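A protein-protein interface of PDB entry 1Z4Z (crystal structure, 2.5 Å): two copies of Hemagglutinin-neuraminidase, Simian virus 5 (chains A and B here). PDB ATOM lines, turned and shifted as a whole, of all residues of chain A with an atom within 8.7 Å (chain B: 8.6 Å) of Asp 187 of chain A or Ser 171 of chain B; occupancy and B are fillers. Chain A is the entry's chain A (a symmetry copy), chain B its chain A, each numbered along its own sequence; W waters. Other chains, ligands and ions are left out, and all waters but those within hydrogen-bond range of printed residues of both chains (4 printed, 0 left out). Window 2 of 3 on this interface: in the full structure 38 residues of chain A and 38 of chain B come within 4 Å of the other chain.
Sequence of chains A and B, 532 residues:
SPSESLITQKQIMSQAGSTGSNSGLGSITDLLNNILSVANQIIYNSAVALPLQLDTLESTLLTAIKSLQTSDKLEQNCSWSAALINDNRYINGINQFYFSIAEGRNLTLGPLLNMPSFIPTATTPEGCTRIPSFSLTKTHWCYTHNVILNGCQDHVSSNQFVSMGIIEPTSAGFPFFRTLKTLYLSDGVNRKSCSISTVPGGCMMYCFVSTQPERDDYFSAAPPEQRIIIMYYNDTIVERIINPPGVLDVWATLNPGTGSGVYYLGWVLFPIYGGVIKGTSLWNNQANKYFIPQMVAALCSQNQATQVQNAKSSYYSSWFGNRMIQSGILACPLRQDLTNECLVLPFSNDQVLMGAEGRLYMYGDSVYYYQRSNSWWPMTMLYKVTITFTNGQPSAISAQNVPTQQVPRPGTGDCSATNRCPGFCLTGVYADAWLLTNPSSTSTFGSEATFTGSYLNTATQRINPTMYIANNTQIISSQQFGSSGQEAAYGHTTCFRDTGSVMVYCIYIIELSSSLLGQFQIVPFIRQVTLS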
ATOM      1  N   LEU A 149      29.917 -14.660 -26.810  1.00  0.00           N
ATOM      2  CA  LEU A 149      30.305 -15.910 -27.457  1.00  0.00           C
ATOM      3  C   LEU A 149      31.784 -16.312 -27.382  1.00  0.00           C
ATOM      4  O   LEU A 149      32.092 -17.480 -27.136  1.00  0.00           O
ATOM      5  CB  LEU A 149      29.831 -15.906 -28.920  1.00  0.00           C
ATOM      6  CG  LEU A 149      28.317 -15.726 -29.124  1.00  0.00           C
ATOM      7  CD1 LEU A 149      27.970 -15.948 -30.601  1.00  0.00           C
ATOM      8  CD2 LEU A 149      27.533 -16.709 -28.237  1.00  0.00           C
ATOM      9  N   VAL A 156      30.699  -4.494 -28.879  1.00  0.00           N
ATOM     10  CA  VAL A 156      29.930  -4.679 -30.126  1.00  0.00           C
ATOM     11  C   VAL A 156      28.725  -5.618 -29.943  1.00  0.00           C
ATOM     12  O   VAL A 156      27.561  -5.208 -30.015  1.00  0.00           O
ATOM     13  CB  VAL A 156      30.851  -5.385 -31.180  1.00  0.00           C
ATOM     14  CG1 VAL A 156      30.150  -5.533 -32.530  1.00  0.00           C
ATOM     15  CG2 VAL A 156      32.176  -4.661 -31.291  1.00  0.00           C
ATOM     16  N   SER A 157      29.058  -6.898 -29.750  1.00  0.00           N
ATOM     17  CA  SER A 157      28.102  -7.998 -29.587  1.00  0.00           C
ATOM     18  C   SER A 157      28.055  -8.638 -28.210  1.00  0.00           C
ATOM     19  O   SER A 157      29.058  -8.739 -27.509  1.00  0.00           O
ATOM     20  CB  SER A 157      28.420  -9.132 -30.574  1.00  0.00           C
ATOM     21  OG  SER A 157      27.430 -10.149 -30.513  1.00  0.00           O
ATOM     22  N   SER A 158      26.868  -9.103 -27.860  1.00  0.00           N
ATOM     23  CA  SER A 158      26.631  -9.799 -26.615  1.00  0.00           C
ATOM     24  C   SER A 158      25.141  -9.964 -26.487  1.00  0.00           C
ATOM     25  O   SER A 158      24.369  -9.223 -27.086  1.00  0.00           O
ATOM     26  CB  SER A 158      27.174  -9.022 -25.409  1.00  0.00           C
ATOM     27  OG  SER A 158      26.210  -8.133 -24.886  1.00  0.00           O
ATOM     28  N   ASN A 159      24.741 -10.961 -25.723  1.00  0.00           N
ATOM     29  CA  ASN A 159      23.332 -11.210 -25.526  1.00  0.00           C
ATOM     30  C   ASN A 159      23.112 -11.171 -24.029  1.00  0.00           C
ATOM     31  O   ASN A 159      24.065 -11.262 -23.259  1.00  0.00           O
ATOM     32  CB  ASN A 159      22.956 -12.569 -26.116  1.00  0.00           C
ATOM     33  CG  ASN A 159      23.277 -12.657 -27.593  1.00  0.00           C
ATOM     34  OD1 ASN A 159      22.924 -11.762 -28.361  1.00  0.00           O
ATOM     35  ND2 ASN A 159      23.946 -13.734 -28.002  1.00  0.00           N
ATOM     36  N   GLN A 160      21.863 -11.016 -23.617  1.00  0.00           N
ATOM     37  CA  GLN A 160      21.551 -10.957 -22.203  1.00  0.00           C
ATOM     38  C   GLN A 160      20.467 -11.976 -21.893  1.00  0.00           C
ATOM     39  O   GLN A 160      19.378 -11.913 -22.452  1.00  0.00           O
ATOM     40  CB  GLN A 160      21.059  -9.561 -21.845  1.00  0.00           C
ATOM     41  CG  GLN A 160      20.875  -9.304 -20.364  1.00  0.00           C
ATOM     42  CD  GLN A 160      22.184  -9.031 -19.655  1.00  0.00           C
ATOM     43  OE1 GLN A 160      23.160  -8.605 -20.269  1.00  0.00           O
ATOM     44  NE2 GLN A 160      22.203  -9.252 -18.350  1.00  0.00           N
ATOM     45  N   TYR A 184      15.953 -14.583 -24.009  1.00  0.00           N
ATOM     46  CA  TYR A 184      17.324 -14.368 -24.442  1.00  0.00           C
ATOM     47  C   TYR A 184      17.318 -13.178 -25.389  1.00  0.00           C
ATOM     48  O   TYR A 184      16.910 -13.294 -26.544  1.00  0.00           O
ATOM     49  CB  TYR A 184      17.868 -15.618 -25.138  1.00  0.00           C
ATOM     50  CG  TYR A 184      19.369 -15.639 -25.354  1.00  0.00           C
ATOM     51  CD1 TYR A 184      20.251 -15.238 -24.345  1.00  0.00           C
ATOM     52  CD2 TYR A 184      19.912 -16.127 -26.545  1.00  0.00           C
ATOM     53  CE1 TYR A 184      21.633 -15.331 -24.516  1.00  0.00           C
ATOM     54  CE2 TYR A 184      21.290 -16.225 -26.730  1.00  0.00           C
ATOM     55  CZ  TYR A 184      22.147 -15.830 -25.716  1.00  0.00           C
ATOM     56  OH  TYR A 184      23.514 -15.948 -25.903  1.00  0.00           O
ATOM     57  N   LEU A 185      17.741 -12.026 -24.877  1.00  0.00           N
ATOM     58  CA  LEU A 185      17.802 -10.804 -25.659  1.00  0.00           C
ATOM     59  C   LEU A 185      19.032 -10.880 -26.553  1.00  0.00           C
ATOM     60  O   LEU A 185      20.161 -10.605 -26.130  1.00  0.00           O
ATOM     61  CB  LEU A 185      17.881  -9.596 -24.730  1.00  0.00           C
ATOM     62  CG  LEU A 185      16.754  -9.563 -23.690  1.00  0.00           C
ATOM     63  CD1 LEU A 185      16.871  -8.307 -22.820  1.00  0.00           C
ATOM     64  CD2 LEU A 185      15.407  -9.591 -24.405  1.00  0.00           C
ATOM     65  N   SER A 186      18.795 -11.274 -27.795  1.00  0.00           N
ATOM     66  CA  SER A 186      19.843 -11.432 -28.787  1.00  0.00           C
ATOM     67  C   SER A 186      19.342 -10.723 -30.041  1.00  0.00           C
ATOM     68  O   SER A 186      18.549 -11.281 -30.792  1.00  0.00           O
ATOM     69  CB  SER A 186      20.040 -12.925 -29.051  1.00  0.00           C
ATOM     70  OG  SER A 186      21.130 -13.158 -29.913  1.00  0.00           O
ATOM     71  N   ASP A 187      19.800  -9.496 -30.270  1.00  0.00           N
ATOM     72  CA  ASP A 187      19.324  -8.745 -31.425  1.00  0.00           C
ATOM     73  C   ASP A 187      20.285  -7.689 -31.959  1.00  0.00           C
ATOM     74  O   ASP A 187      19.892  -6.852 -32.771  1.00  0.00           O
ATOM     75  CB  ASP A 187      17.998  -8.068 -31.072  1.00  0.00           C
ATOM     76  CG  ASP A 187      18.166  -6.978 -30.028  1.00  0.00           C
ATOM     77  OD1 ASP A 187      19.299  -6.823 -29.519  1.00  0.00           O
ATOM     78  OD2 ASP A 187      17.179  -6.282 -29.715  1.00  0.00           O
ATOM     79  N   GLY A 188      21.532  -7.710 -31.508  1.00  0.00           N
ATOM     80  CA  GLY A 188      22.482  -6.726 -31.995  1.00  0.00           C
ATOM     81  C   GLY A 188      22.714  -5.540 -31.073  1.00  0.00           C
ATOM     82  O   GLY A 188      23.710  -4.828 -31.216  1.00  0.00           O
ATOM     83  N   VAL A 189      21.797  -5.301 -30.142  1.00  0.00           N
ATOM     84  CA  VAL A 189      21.976  -4.204 -29.202  1.00  0.00           C
ATOM     85  C   VAL A 189      22.864  -4.717 -28.070  1.00  0.00           C
ATOM     86  O   VAL A 189      22.503  -5.656 -27.365  1.00  0.00           O
ATOM     87  CB  VAL A 189      20.634  -3.732 -28.638  1.00  0.00           C
ATOM     88  CG1 VAL A 189      20.860  -2.691 -27.561  1.00  0.00           C
ATOM     89  CG2 VAL A 189      19.796  -3.146 -29.760  1.00  0.00           C
ATOM     90  N   ASN A 190      24.030  -4.105 -27.906  1.00  0.00           N
ATOM     91  CA  ASN A 190      24.979  -4.532 -26.883  1.00  0.00           C
ATOM     92  C   ASN A 190      24.660  -3.989 -25.484  1.00  0.00           C
ATOM     93  O   ASN A 190      25.281  -3.034 -25.004  1.00  0.00           O
ATOM     94  CB  ASN A 190      26.394  -4.134 -27.319  1.00  0.00           C
ATOM     95  CG  ASN A 190      27.471  -4.927 -26.610  1.00  0.00           C
ATOM     96  OD1 ASN A 190      27.288  -6.098 -26.290  1.00  0.00           O
ATOM     97  ND2 ASN A 190      28.612  -4.298 -26.383  1.00  0.00           N
ATOM     98  N   ARG A 191      23.677  -4.616 -24.843  1.00  0.00           N
ATOM     99  CA  ARG A 191      23.241  -4.250 -23.497  1.00  0.00           C
ATOM    100  C   ARG A 191      24.235  -4.763 -22.464  1.00  0.00           C
ATOM    101  O   ARG A 191      24.492  -5.961 -22.382  1.00  0.00           O
ATOM    102  CB  ARG A 191      21.848  -4.831 -23.239  1.00  0.00           C
ATOM    103  CG  ARG A 191      20.737  -4.006 -23.884  1.00  0.00           C
ATOM    104  CD  ARG A 191      19.410  -4.730 -23.927  1.00  0.00           C
ATOM    105  NE  ARG A 191      19.413  -5.699 -25.009  1.00  0.00           N
ATOM    106  CZ  ARG A 191      18.590  -5.667 -26.049  1.00  0.00           C
ATOM    107  NH1 ARG A 191      17.677  -4.714 -26.162  1.00  0.00           N
ATOM    108  NH2 ARG A 191      18.701  -6.587 -26.991  1.00  0.00           N
ATOM    109  N   VAL A 209      23.875   0.795 -23.496  1.00  0.00           N
ATOM    110  CA  VAL A 209      24.401   0.173 -24.708  1.00  0.00           C
ATOM    111  C   VAL A 209      25.872   0.506 -24.928  1.00  0.00           C
ATOM    112  O   VAL A 209      26.236   1.666 -25.162  1.00  0.00           O
ATOM    113  CB  VAL A 209      23.589   0.603 -25.941  1.00  0.00           C
ATOM    114  CG1 VAL A 209      24.076  -0.139 -27.167  1.00  0.00           C
ATOM    115  CG2 VAL A 209      22.122   0.324 -25.706  1.00  0.00           C
ATOM    116  N   ARG A 227      18.814   2.219 -21.512  1.00  0.00           N
ATOM    117  CA  ARG A 227      17.565   1.513 -21.788  1.00  0.00           C
ATOM    118  C   ARG A 227      16.976   0.778 -20.597  1.00  0.00           C
ATOM    119  O   ARG A 227      17.699   0.249 -19.754  1.00  0.00           O
ATOM    120  CB  ARG A 227      17.763   0.497 -22.908  1.00  0.00           C
ATOM    121  CG  ARG A 227      18.170   1.091 -24.236  1.00  0.00           C
ATOM    122  CD  ARG A 227      18.214   0.013 -25.301  1.00  0.00           C
ATOM    123  NE  ARG A 227      18.431   0.567 -26.632  1.00  0.00           N
ATOM    124  CZ  ARG A 227      17.892   0.069 -27.739  1.00  0.00           C
ATOM    125  NH1 ARG A 227      17.102  -0.993 -27.663  1.00  0.00           N
ATOM    126  NH2 ARG A 227      18.141   0.631 -28.916  1.00  0.00           N
ATOM    127  N   ILE A 229      14.083  -2.183 -19.891  1.00  0.00           N
ATOM    128  CA  ILE A 229      13.203  -3.181 -20.488  1.00  0.00           C
ATOM    129  C   ILE A 229      12.291  -3.772 -19.416  1.00  0.00           C
ATOM    130  O   ILE A 229      12.761  -4.193 -18.354  1.00  0.00           O
ATOM    131  CB  ILE A 229      14.003  -4.364 -21.123  1.00  0.00           C
ATOM    132  CG1 ILE A 229      15.058  -3.850 -22.103  1.00  0.00           C
ATOM    133  CG2 ILE A 229      13.068  -5.280 -21.883  1.00  0.00           C
ATOM    134  CD1 ILE A 229      16.354  -3.378 -21.454  1.00  0.00           C
ATOM    135  N   GLU A 239      10.569  -2.252 -24.316  1.00  0.00           N
ATOM    136  CA  GLU A 239      11.870  -1.650 -24.091  1.00  0.00           C
ATOM    137  C   GLU A 239      11.798  -0.180 -24.480  1.00  0.00           C
ATOM    138  O   GLU A 239      11.180   0.177 -25.480  1.00  0.00           O
ATOM    139  CB  GLU A 239      12.949  -2.373 -24.904  1.00  0.00           C
ATOM    140  CG  GLU A 239      14.321  -1.711 -24.820  1.00  0.00           C
ATOM    141  CD  GLU A 239      15.453  -2.605 -25.307  1.00  0.00           C
ATOM    142  OE1 GLU A 239      15.313  -3.219 -26.390  1.00  0.00           O
ATOM    143  OE2 GLU A 239      16.487  -2.684 -24.606  1.00  0.00           O
ATOM    144  N   ARG B  89      11.184 -21.067 -38.105  1.00  0.00           N
ATOM    145  CA  ARG B  89      12.414 -21.556 -38.683  1.00  0.00           C
ATOM    146  C   ARG B  89      12.668 -23.031 -38.399  1.00  0.00           C
ATOM    147  O   ARG B  89      13.532 -23.643 -39.029  1.00  0.00           O
ATOM    148  CB  ARG B  89      13.584 -20.739 -38.161  1.00  0.00           C
ATOM    149  CG  ARG B  89      13.667 -19.361 -38.773  1.00  0.00           C
ATOM    150  CD  ARG B  89      15.065 -19.151 -39.287  1.00  0.00           C
ATOM    151  NE  ARG B  89      15.619 -17.892 -38.824  1.00  0.00           N
ATOM    152  CZ  ARG B  89      16.903 -17.702 -38.558  1.00  0.00           C
ATOM    153  NH1 ARG B  89      17.769 -18.700 -38.710  1.00  0.00           N
ATOM    154  NH2 ARG B  89      17.315 -16.510 -38.145  1.00  0.00           N
ATOM    155  N   GLU B 168      14.180 -21.111 -30.721  1.00  0.00           N
ATOM    156  CA  GLU B 168      14.100 -19.851 -31.442  1.00  0.00           C
ATOM    157  C   GLU B 168      15.492 -19.411 -31.849  1.00  0.00           C
ATOM    158  O   GLU B 168      16.469 -19.699 -31.167  1.00  0.00           O
ATOM    159  CB  GLU B 168      13.432 -18.764 -30.594  1.00  0.00           C
ATOM    160  CG  GLU B 168      14.148 -18.421 -29.315  1.00  0.00           C
ATOM    161  CD  GLU B 168      13.537 -17.210 -28.628  1.00  0.00           C
ATOM    162  OE1 GLU B 168      12.288 -17.130 -28.576  1.00  0.00           O
ATOM    163  OE2 GLU B 168      14.302 -16.345 -28.134  1.00  0.00           O
ATOM    164  N   PRO B 169      15.600 -18.701 -32.977  1.00  0.00           N
ATOM    165  CA  PRO B 169      16.895 -18.229 -33.473  1.00  0.00           C
ATOM    166  C   PRO B 169      17.498 -17.073 -32.689  1.00  0.00           C
ATOM    167  O   PRO B 169      16.779 -16.224 -32.162  1.00  0.00           O
ATOM    168  CB  PRO B 169      16.582 -17.844 -34.912  1.00  0.00           C
ATOM    169  CG  PRO B 169      15.185 -17.303 -34.794  1.00  0.00           C
ATOM    170  CD  PRO B 169      14.509 -18.312 -33.890  1.00  0.00           C
ATOM    171  N   THR B 170      18.825 -17.061 -32.606  1.00  0.00           N
ATOM    172  CA  THR B 170      19.551 -16.000 -31.921  1.00  0.00           C
ATOM    173  C   THR B 170      20.076 -15.078 -33.017  1.00  0.00           C
ATOM    174  O   THR B 170      20.049 -15.435 -34.193  1.00  0.00           O
ATOM    175  CB  THR B 170      20.740 -16.548 -31.117  1.00  0.00           C
ATOM    176  OG1 THR B 170      21.696 -17.137 -32.008  1.00  0.00           O
ATOM    177  CG2 THR B 170      20.272 -17.597 -30.137  1.00  0.00           C
ATOM    178  N   SER B 171      20.555 -13.899 -32.642  1.00  0.00           N
ATOM    179  CA  SER B 171      21.060 -12.961 -33.638  1.00  0.00           C
ATOM    180  C   SER B 171      22.243 -13.527 -34.433  1.00  0.00           C
ATOM    181  O   SER B 171      22.557 -13.038 -35.521  1.00  0.00           O
ATOM    182  CB  SER B 171      21.463 -11.646 -32.970  1.00  0.00           C
ATOM    183  OG  SER B 171      22.620 -11.812 -32.173  1.00  0.00           O
ATOM    184  N   ALA B 172      22.895 -14.555 -33.895  1.00  0.00           N
ATOM    185  CA  ALA B 172      24.036 -15.162 -34.576  1.00  0.00           C
ATOM    186  C   ALA B 172      23.558 -16.211 -35.559  1.00  0.00           C
ATOM    187  O   ALA B 172      24.353 -16.796 -36.296  1.00  0.00           O
ATOM    188  CB  ALA B 172      24.981 -15.792 -33.571  1.00  0.00           C
ATOM    189  N   GLY B 173      22.256 -16.458 -35.560  1.00  0.00           N
ATOM    190  CA  GLY B 173      21.709 -17.438 -36.471  1.00  0.00           C
ATOM    191  C   GLY B 173      21.465 -18.814 -35.885  1.00  0.00           C
ATOM    192  O   GLY B 173      20.611 -19.538 -36.389  1.00  0.00           O
ATOM    193  N   PHE B 174      22.186 -19.204 -34.837  1.00  0.00           N
ATOM    194  CA  PHE B 174      21.938 -20.533 -34.301  1.00  0.00           C
ATOM    195  C   PHE B 174      20.874 -20.587 -33.209  1.00  0.00           C
ATOM    196  O   PHE B 174      20.520 -19.573 -32.617  1.00  0.00           O
ATOM    197  CB  PHE B 174      23.254 -21.214 -33.878  1.00  0.00           C
ATOM    198  CG  PHE B 174      24.080 -20.445 -32.902  1.00  0.00           C
ATOM    199  CD1 PHE B 174      23.778 -20.468 -31.541  1.00  0.00           C
ATOM    200  CD2 PHE B 174      25.213 -19.760 -33.331  1.00  0.00           C
ATOM    201  CE1 PHE B 174      24.601 -19.821 -30.613  1.00  0.00           C
ATOM    202  CE2 PHE B 174      26.042 -19.109 -32.420  1.00  0.00           C
ATOM    203  CZ  PHE B 174      25.739 -19.141 -31.056  1.00  0.00           C
ATOM    204  N   PRO B 175      20.328 -21.786 -32.953  1.00  0.00           N
ATOM    205  CA  PRO B 175      19.283 -22.044 -31.961  1.00  0.00           C
ATOM    206  C   PRO B 175      19.542 -21.697 -30.506  1.00  0.00           C
ATOM    207  O   PRO B 175      20.674 -21.691 -30.031  1.00  0.00           O
ATOM    208  CB  PRO B 175      19.018 -23.545 -32.111  1.00  0.00           C
ATOM    209  CG  PRO B 175      19.466 -23.856 -33.485  1.00  0.00           C
ATOM    210  CD  PRO B 175      20.721 -23.046 -33.608  1.00  0.00           C
ATOM    211  N   PHE B 176      18.444 -21.413 -29.817  1.00  0.00           N
ATOM    212  CA  PHE B 176      18.430 -21.135 -28.396  1.00  0.00           C
ATOM    213  C   PHE B 176      17.239 -21.935 -27.900  1.00  0.00           C
ATOM    214  O   PHE B 176      16.128 -21.758 -28.386  1.00  0.00           O
ATOM    215  CB  PHE B 176      18.202 -19.650 -28.094  1.00  0.00           C
ATOM    216  CG  PHE B 176      17.703 -19.391 -26.688  1.00  0.00           C
ATOM    217  CD1 PHE B 176      18.309 -20.008 -25.592  1.00  0.00           C
ATOM    218  CD2 PHE B 176      16.614 -18.553 -26.462  1.00  0.00           C
ATOM    219  CE1 PHE B 176      17.839 -19.801 -24.298  1.00  0.00           C
ATOM    220  CE2 PHE B 176      16.134 -18.336 -25.168  1.00  0.00           C
ATOM    221  CZ  PHE B 176      16.748 -18.963 -24.083  1.00  0.00           C
HETATM  222  O   HOH W   1      24.145 -14.036 -30.835  1.00  0.00           O
HETATM  223  O   HOH W   2      13.498 -14.811 -26.009  1.00  0.00           O
HETATM  224  O   HOH W   3      16.365 -14.746 -28.859  1.00  0.00           O
HETATM  225  O   HOH W   4      23.702  -9.982 -30.422  1.00  0.00           O
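The side-chain hydroxyl (OG) of Ser 186 of chain A lies within hydrogen-bond range of the backbone NH (N) of Ser 171 of chain B (2.9 Å).
The backbone carbonyl oxygen (O) of Glu 168 of chain B lies within hydrogen-bond range of the backbone NH (N) of Phe 176 of chain B.
OG1 of Thr 170 of chain B is in hydrogen-bond range of O of Phe 174 of chain B (2.8 Å).
OH of Tyr 184 of chain A sits at hydrogen-bond distance from ND2 of Asn 159 of chain A (3.1 Å).
The side-chain amide oxygen (OD1) of Asn 159 of chain A sits at hydrogen-bond distance from the side-chain hydroxyl (OG) of Ser 186 of chain A.
OD1 of Asp 187 of chain A is in hydrogen-bond range of N of Val 189 of chain A, 3.0 Å away.
NH2 of Arg 191 of chain A lies within salt-bridge range of OD1 of Asp 187 of chain A (2.6 Å).
CZ of Phe 174 of chain B touches CD1 of Leu 149 of chain A, at 3.9 Å.
OD1 of Asn 159 of chain A touches OG of Ser 171 of chain B, 3.8 Å away.
CG2 of Thr 170 of chain B touches CE2 of Tyr 184 of chain A (3.8 Å).
CE2 of Phe 176 of chain B touches CB of Tyr 184 of chain A, 3.2 Å away.
OG of Ser 186 of chain A touches CB of Thr 170 of chain B (3.6 Å).
N of Asp 187 of chain A touches CB of Ser 171 of chain B, at 3.8 Å.
Of the printed residues of chain B, Tyr 184 of chain A touches Thr 170 (3.8 Å) and Phe 176 (3.2 Å).
Of chain B, only Thr 170 and Ser 171 come within 4 Å of Ser 186 of chain A.
Of chain B, only Ser 171 comes within 4 Å of Asp 187 of chain A.
Glu 239 of chain A touches none of the printed residues of chain B.
Pro 169 of chain B touches none of the printed residues of chain A.
Of chain A, only Asn 159 (3.8 Å), Ser 186 (2.9 Å) and Asp 187 (3.8 Å) come within 4 Å of Ser 171 of chain B.
Printed residues of chain A within 4 Å of Phe 176 of chain B: Tyr 184.
The nearest residue of chain B that does not touch Asp 187 of chain A is Thr 170 of chain B (6.2 Å).
The nearest residue of chain A that does not touch Ser 171 of chain B is Gly 188 of chain A (4.2 Å).
The nearest printed residue of chain A that does not touch Phe 174 of chain B is Tyr 184 of chain A (6.2 Å).
Hydrophobic or aromatic side chains of chain A that line the printed part of chain B: Leu 149 and Tyr 184.
Of the 10 printed residues of chain B, 4 touch a printed residue of chain A.
Among the printed residues, no Asp or Glu carboxylate lies within 4 Å of a Lys or Arg side-chain nitrogen of the other chain.
No position is printed for both chains.
Water W3 bridges OE2 of Glu 168 of chain B (2.7 Å) and O of Tyr 184 of chain A (2.8 Å).
Water W2 lies within hydrogen-bond range of the side-chain carboxylate (OE2) of Glu 168 of chain B (2.7 Å) and the backbone NH (N) of Tyr 184 of chain A (3.2 Å).
Water W4 lies within hydrogen-bond range of OG of Ser 171 of chain B (2.8 Å), OD1 of Asn 159 of chain A (2.8 Å), N of Gly 188 of chain A (3.3 Å) and O of Ser 158 of chain A (3.5 Å).
Water W1 lies within hydrogen-bond range of ND2 of Asn 159 of chain A (2.9 Å), OG of Ser 171 of chain B (3.0 Å), OG of Ser 186 of chain A (3.3 Å) and N of Ala 172 of chain B (3.3 Å).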
